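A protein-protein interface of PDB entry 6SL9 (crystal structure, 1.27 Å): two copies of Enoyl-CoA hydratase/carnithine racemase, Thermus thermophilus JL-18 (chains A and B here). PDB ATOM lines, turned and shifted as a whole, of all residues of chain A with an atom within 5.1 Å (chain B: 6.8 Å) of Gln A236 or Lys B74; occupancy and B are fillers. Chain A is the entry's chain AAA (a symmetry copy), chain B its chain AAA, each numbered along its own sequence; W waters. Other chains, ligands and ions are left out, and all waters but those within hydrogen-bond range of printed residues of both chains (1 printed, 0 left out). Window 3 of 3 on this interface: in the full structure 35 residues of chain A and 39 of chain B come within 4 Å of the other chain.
The side-chain amide nitrogen of Gln A236 sits at hydrogen-bond distance from the backbone carbonyl oxygen of Gly A232, at 3.3 Å. The backbone carbonyl oxygen of Ala A234 is in hydrogen-bond range of the side-chain hydroxyl of Thr A237.
Gln A231 touches Tyr B77. Gln A231 touches Leu B137 (OE1 to CB, 3.3 Å). Leu B137 touches Ala A234 (CD2 to CB, 3.97 Å). Gly A235 touches Pro B75. Gly A235 touches Tyr B77 (CA to CD2, 3.6 Å). N of Gly A235 touches CD2 of Leu B137 (3.95 Å). Gln A236 touches Lys B74 (OE1 to CE, 2.8 Å).
Of the printed residues of chain B, Gln A231 touches Tyr B77 (3.8 Å) and Leu B137 (3.3 Å). Gly A232 touches none of the printed residues of chain B. Of the printed residues of chain B, Ala A234 touches Leu B137. Gly A235 touches just these residues of chain B: Pro B75 (3.3 Å), Tyr B77 (3.6 Å) and Leu B137 (3.95 Å). Of chain B, only Lys B74 comes within 4 Å of Gln A236. Gly B71 touches none of the printed residues of chain A. Printed residues of chain A within 4 Å of Lys B74: Gln A236 (2.8 Å). Printed residues of chain A within 4 Å of Pro B75: Gly A235 (3.3 Å). Of the printed residues of chain A, Leu B137 touches Gln A231, Ala A234 and Gly A235. The nearest residue of chain B that does not touch Gln A236 is Pro B75 (4.1 Å). The nearest printed residue of chain A that does not touch Lys B74 is Gly A235 (5.2 Å).
Of the 8 printed residues of chain B, 4 touch a printed residue of chain A. Hydrophobic or aromatic side chains of chain B within 4 Å of the printed part of chain A: Pro B75, Tyr B77 and Leu B137. Printed residues of chain A that touch a printed residue of chain B: Gln A231, Ala A234, Gly A235 and Gln A236. Hydrophobic or aromatic side chains of chain A within 4 Å of the printed part of chain B: Ala A234. Among the printed residues, 7 pairs touch across the chains. Among the printed residues, no Asp or Glu carboxylate lies within 4 Å of a Lys or Arg side-chain nitrogen of the other chain.
No position is printed for both chains. Of the 7 pairs that touch across the chains among the printed residues, none has its exchanged pair printed and touching as well.
Water W1 lies within hydrogen-bond range of O of Pro B75 (2.8 Å), O of Gly A232 (2.8 Å) and N of Tyr B77 (3.0 Å).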
ATOM      1  N   GLN A 231      21.306 -10.874 -17.365  1.00  0.00           N
ATOM      2  CA  GLN A 231      20.084 -10.164 -16.968  1.00  0.00           C
ATOM      3  C   GLN A 231      18.851 -10.935 -17.430  1.00  0.00           C
ATOM      4  O   GLN A 231      17.825 -10.915 -16.711  1.00  0.00           O
ATOM      5  CB  GLN A 231      20.048  -8.757 -17.531  1.00  0.00           C
ATOM      6  CG  GLN A 231      19.014  -7.834 -16.898  1.00  0.00           C
ATOM      7  CD  GLN A 231      19.463  -7.432 -15.504  1.00  0.00           C
ATOM      8  OE1 GLN A 231      19.558  -8.269 -14.572  1.00  0.00           O
ATOM      9  NE2 GLN A 231      19.855  -6.172 -15.403  1.00  0.00           N
ATOM     10  N   GLY A 232      18.907 -11.591 -18.551  1.00  0.00           N
ATOM     11  CA  GLY A 232      17.773 -12.420 -19.005  1.00  0.00           C
ATOM     12  C   GLY A 232      17.476 -13.465 -17.965  1.00  0.00           C
ATOM     13  O   GLY A 232      16.302 -13.725 -17.609  1.00  0.00           O
ATOM     14  N   GLN A 233      18.522 -14.107 -17.444  1.00  0.00           N
ATOM     15  CA  GLN A 233      18.376 -15.126 -16.375  1.00  0.00           C
ATOM     16  C   GLN A 233      17.837 -14.459 -15.110  1.00  0.00           C
ATOM     17  O   GLN A 233      16.877 -14.998 -14.507  1.00  0.00           O
ATOM     18  CB  GLN A 233      19.696 -15.824 -16.132  1.00  0.00           C
ATOM     19  CG  GLN A 233      20.189 -16.610 -17.325  1.00  0.00           C
ATOM     20  CD  GLN A 233      21.535 -17.254 -17.149  1.00  0.00           C
ATOM     21  OE1 GLN A 233      22.063 -17.341 -16.042  1.00  0.00           O
ATOM     22  NE2 GLN A 233      22.147 -17.643 -18.274  1.00  0.00           N
ATOM     23  N   ALA A 234      18.437 -13.377 -14.657  1.00  0.00           N
ATOM     24  CA  ALA A 234      17.980 -12.729 -13.416  1.00  0.00           C
ATOM     25  C   ALA A 234      16.501 -12.285 -13.533  1.00  0.00           C
ATOM     26  O   ALA A 234      15.720 -12.406 -12.584  1.00  0.00           O
ATOM     27  CB  ALA A 234      18.851 -11.545 -13.052  1.00  0.00           C
ATOM     28  N   GLY A 235      16.080 -11.868 -14.705  1.00  0.00           N
ATOM     29  CA  GLY A 235      14.729 -11.363 -14.950  1.00  0.00           C
ATOM     30  C   GLY A 235      13.695 -12.464 -14.847  1.00  0.00           C
ATOM     31  O   GLY A 235      12.525 -12.132 -14.647  1.00  0.00           O
ATOM     32  N   GLN A 236      14.101 -13.727 -14.977  1.00  0.00           N
ATOM     33  CA  GLN A 236      13.151 -14.848 -14.929  1.00  0.00           C
ATOM     34  C   GLN A 236      13.034 -15.424 -13.519  1.00  0.00           C
ATOM     35  O   GLN A 236      12.229 -16.308 -13.295  1.00  0.00           O
ATOM     36  CB  GLN A 236      13.598 -15.944 -15.877  1.00  0.00           C
ATOM     37  CG  GLN A 236      13.466 -15.554 -17.335  1.00  0.00           C
ATOM     38  CD  GLN A 236      13.888 -16.681 -18.220  1.00  0.00           C
ATOM     39  OE1 GLN A 236      13.145 -17.626 -18.404  1.00  0.00           O
ATOM     40  NE2 GLN A 236      15.085 -16.562 -18.788  1.00  0.00           N
ATOM     41  N   THR A 237      13.762 -14.876 -12.558  1.00  0.00           N
ATOM     42  CA  THR A 237      13.738 -15.387 -11.182  1.00  0.00           C
ATOM     43  C   THR A 237      12.442 -14.949 -10.463  1.00  0.00           C
ATOM     44  O   THR A 237      11.905 -13.837 -10.685  1.00  0.00           O
ATOM     45  CB  THR A 237      14.976 -14.975 -10.360  1.00  0.00           C
ATOM     46  OG1 THR A 237      15.020 -13.543 -10.235  1.00  0.00           O
ATOM     47  CG2 THR A 237      16.253 -15.538 -10.944  1.00  0.00           C
ATOM     48  N   GLN A 238      12.040 -15.744  -9.493  1.00  0.00           N
ATOM     49  CA  GLN A 238      10.958 -15.338  -8.579  1.00  0.00           C
ATOM     50  C   GLN A 238      11.371 -14.090  -7.812  1.00  0.00           C
ATOM     51  O   GLN A 238      10.545 -13.194  -7.602  1.00  0.00           O
ATOM     52  CB  GLN A 238      10.668 -16.479  -7.617  1.00  0.00           C
ATOM     53  CG  GLN A 238      10.199 -17.743  -8.272  1.00  0.00           C
ATOM     54  CD  GLN A 238       8.796 -17.640  -8.823  1.00  0.00           C
ATOM     55  OE1 GLN A 238       8.553 -17.970  -9.984  1.00  0.00           O
ATOM     56  NE2 GLN A 238       7.851 -17.181  -8.003  1.00  0.00           N
ATOM     57  N   GLY B  71       5.229  -5.661 -19.682  1.00  0.00           N
ATOM     58  CA  GLY B  71       3.897  -6.122 -19.293  1.00  0.00           C
ATOM     59  C   GLY B  71       3.990  -6.818 -17.955  1.00  0.00           C
ATOM     60  O   GLY B  71       4.977  -6.624 -17.214  1.00  0.00           O
ATOM     61  N   ASP B  72       2.963  -7.603 -17.671  1.00  0.00           N
ATOM     62  CA  ASP B  72       2.910  -8.542 -16.531  1.00  0.00           C
ATOM     63  C   ASP B  72       3.514  -9.869 -17.031  1.00  0.00           C
ATOM     64  O   ASP B  72       3.828 -10.672 -16.189  1.00  0.00           O
ATOM     65  CB  ASP B  72       1.481  -8.586 -15.937  1.00  0.00           C
ATOM     66  CG  ASP B  72       1.075  -7.384 -15.073  1.00  0.00           C
ATOM     67  OD1 ASP B  72       0.990  -6.247 -15.612  1.00  0.00           O
ATOM     68  OD2 ASP B  72       0.798  -7.586 -13.848  1.00  0.00           O
ATOM     69  N   ARG B  73       3.754 -10.051 -18.347  1.00  0.00           N
ATOM     70  CA  ARG B  73       4.390 -11.272 -18.951  1.00  0.00           C
ATOM     71  C   ARG B  73       5.767 -11.514 -18.294  1.00  0.00           C
ATOM     72  O   ARG B  73       6.365 -10.532 -17.740  1.00  0.00           O
ATOM     73  CB  ARG B  73       4.496 -11.165 -20.482  1.00  0.00           C
ATOM     74  CG  ARG B  73       4.889  -9.775 -20.978  1.00  0.00           C
ATOM     75  CD  ARG B  73       5.518  -9.708 -22.361  1.00  0.00           C
ATOM     76  NE  ARG B  73       4.605 -10.111 -23.430  1.00  0.00           N
ATOM     77  CZ  ARG B  73       4.001  -9.300 -24.315  1.00  0.00           C
ATOM     78  NH1 ARG B  73       3.190  -9.844 -25.220  1.00  0.00           N
ATOM     79  NH2 ARG B  73       4.174  -7.973 -24.287  1.00  0.00           N
ATOM     80  N   LYS B  74       6.233 -12.784 -18.239  1.00  0.00           N
ATOM     81  CA  LYS B  74       7.631 -13.086 -17.827  1.00  0.00           C
ATOM     82  C   LYS B  74       8.532 -12.235 -18.711  1.00  0.00           C
ATOM     83  O   LYS B  74       8.433 -12.451 -19.922  1.00  0.00           O
ATOM     84  CB  LYS B  74       7.979 -14.557 -18.085  1.00  0.00           C
ATOM     85  CG  LYS B  74       9.316 -15.046 -17.533  1.00  0.00           C
ATOM     86  CD  LYS B  74       9.823 -16.308 -18.230  1.00  0.00           C
ATOM     87  CE  LYS B  74      10.557 -17.270 -17.318  1.00  0.00           C
ATOM     88  NZ  LYS B  74       9.634 -18.133 -16.545  1.00  0.00           N
ATOM     89  N   PRO B  75       9.372 -11.292 -18.196  1.00  0.00           N
ATOM     90  CA  PRO B  75      10.215 -10.464 -19.068  1.00  0.00           C
ATOM     91  C   PRO B  75      11.332 -11.236 -19.762  1.00  0.00           C
ATOM     92  O   PRO B  75      11.826 -12.282 -19.279  1.00  0.00           O
ATOM     93  CB  PRO B  75      10.912  -9.451 -18.174  1.00  0.00           C
ATOM     94  CG  PRO B  75      10.970 -10.220 -16.846  1.00  0.00           C
ATOM     95  CD  PRO B  75       9.676 -11.022 -16.781  1.00  0.00           C
ATOM     96  N   ASP B  76      11.733 -10.665 -20.886  1.00  0.00           N
ATOM     97  CA  ASP B  76      12.832 -11.170 -21.720  1.00  0.00           C
ATOM     98  C   ASP B  76      13.880 -10.063 -21.748  1.00  0.00           C
ATOM     99  O   ASP B  76      14.027  -9.330 -22.758  1.00  0.00           O
ATOM    100  CB  ASP B  76      12.312 -11.541 -23.089  1.00  0.00           C
ATOM    101  CG  ASP B  76      13.316 -12.216 -24.012  1.00  0.00           C
ATOM    102  OD1 ASP B  76      14.489 -12.277 -23.694  1.00  0.00           O
ATOM    103  OD2 ASP B  76      12.855 -12.710 -25.044  1.00  0.00           O
ATOM    104  N   TYR B  77      14.669  -9.959 -20.697  1.00  0.00           N
ATOM    105  CA  TYR B  77      15.673  -8.888 -20.657  1.00  0.00           C
ATOM    106  C   TYR B  77      16.815  -9.135 -21.639  1.00  0.00           C
ATOM    107  O   TYR B  77      17.460  -8.173 -22.053  1.00  0.00           O
ATOM    108  CB  TYR B  77      16.169  -8.653 -19.250  1.00  0.00           C
ATOM    109  CG  TYR B  77      15.059  -8.116 -18.386  1.00  0.00           C
ATOM    110  CD1 TYR B  77      14.001  -7.358 -18.884  1.00  0.00           C
ATOM    111  CD2 TYR B  77      14.985  -8.471 -17.083  1.00  0.00           C
ATOM    112  CE1 TYR B  77      13.012  -6.899 -18.037  1.00  0.00           C
ATOM    113  CE2 TYR B  77      14.056  -7.983 -16.201  1.00  0.00           C
ATOM    114  CZ  TYR B  77      13.046  -7.237 -16.705  1.00  0.00           C
ATOM    115  OH  TYR B  77      12.068  -6.817 -15.872  1.00  0.00           O
ATOM    116  N   LEU B 137      18.279  -7.855  -9.809  1.00  0.00           N
ATOM    117  CA  LEU B 137      18.914  -7.838 -11.138  1.00  0.00           C
ATOM    118  C   LEU B 137      20.414  -7.636 -11.012  1.00  0.00           C
ATOM    119  O   LEU B 137      20.924  -7.312  -9.950  1.00  0.00           O
ATOM    120  CB  LEU B 137      18.255  -6.739 -11.968  1.00  0.00           C
ATOM    121  CG  LEU B 137      16.795  -6.947 -12.384  1.00  0.00           C
ATOM    122  CD1 LEU B 137      16.373  -5.845 -13.354  1.00  0.00           C
ATOM    123  CD2 LEU B 137      16.547  -8.312 -13.044  1.00  0.00           C
HETATM  124  O   HOH W   1      14.393 -11.733 -18.311  1.00  0.00           O
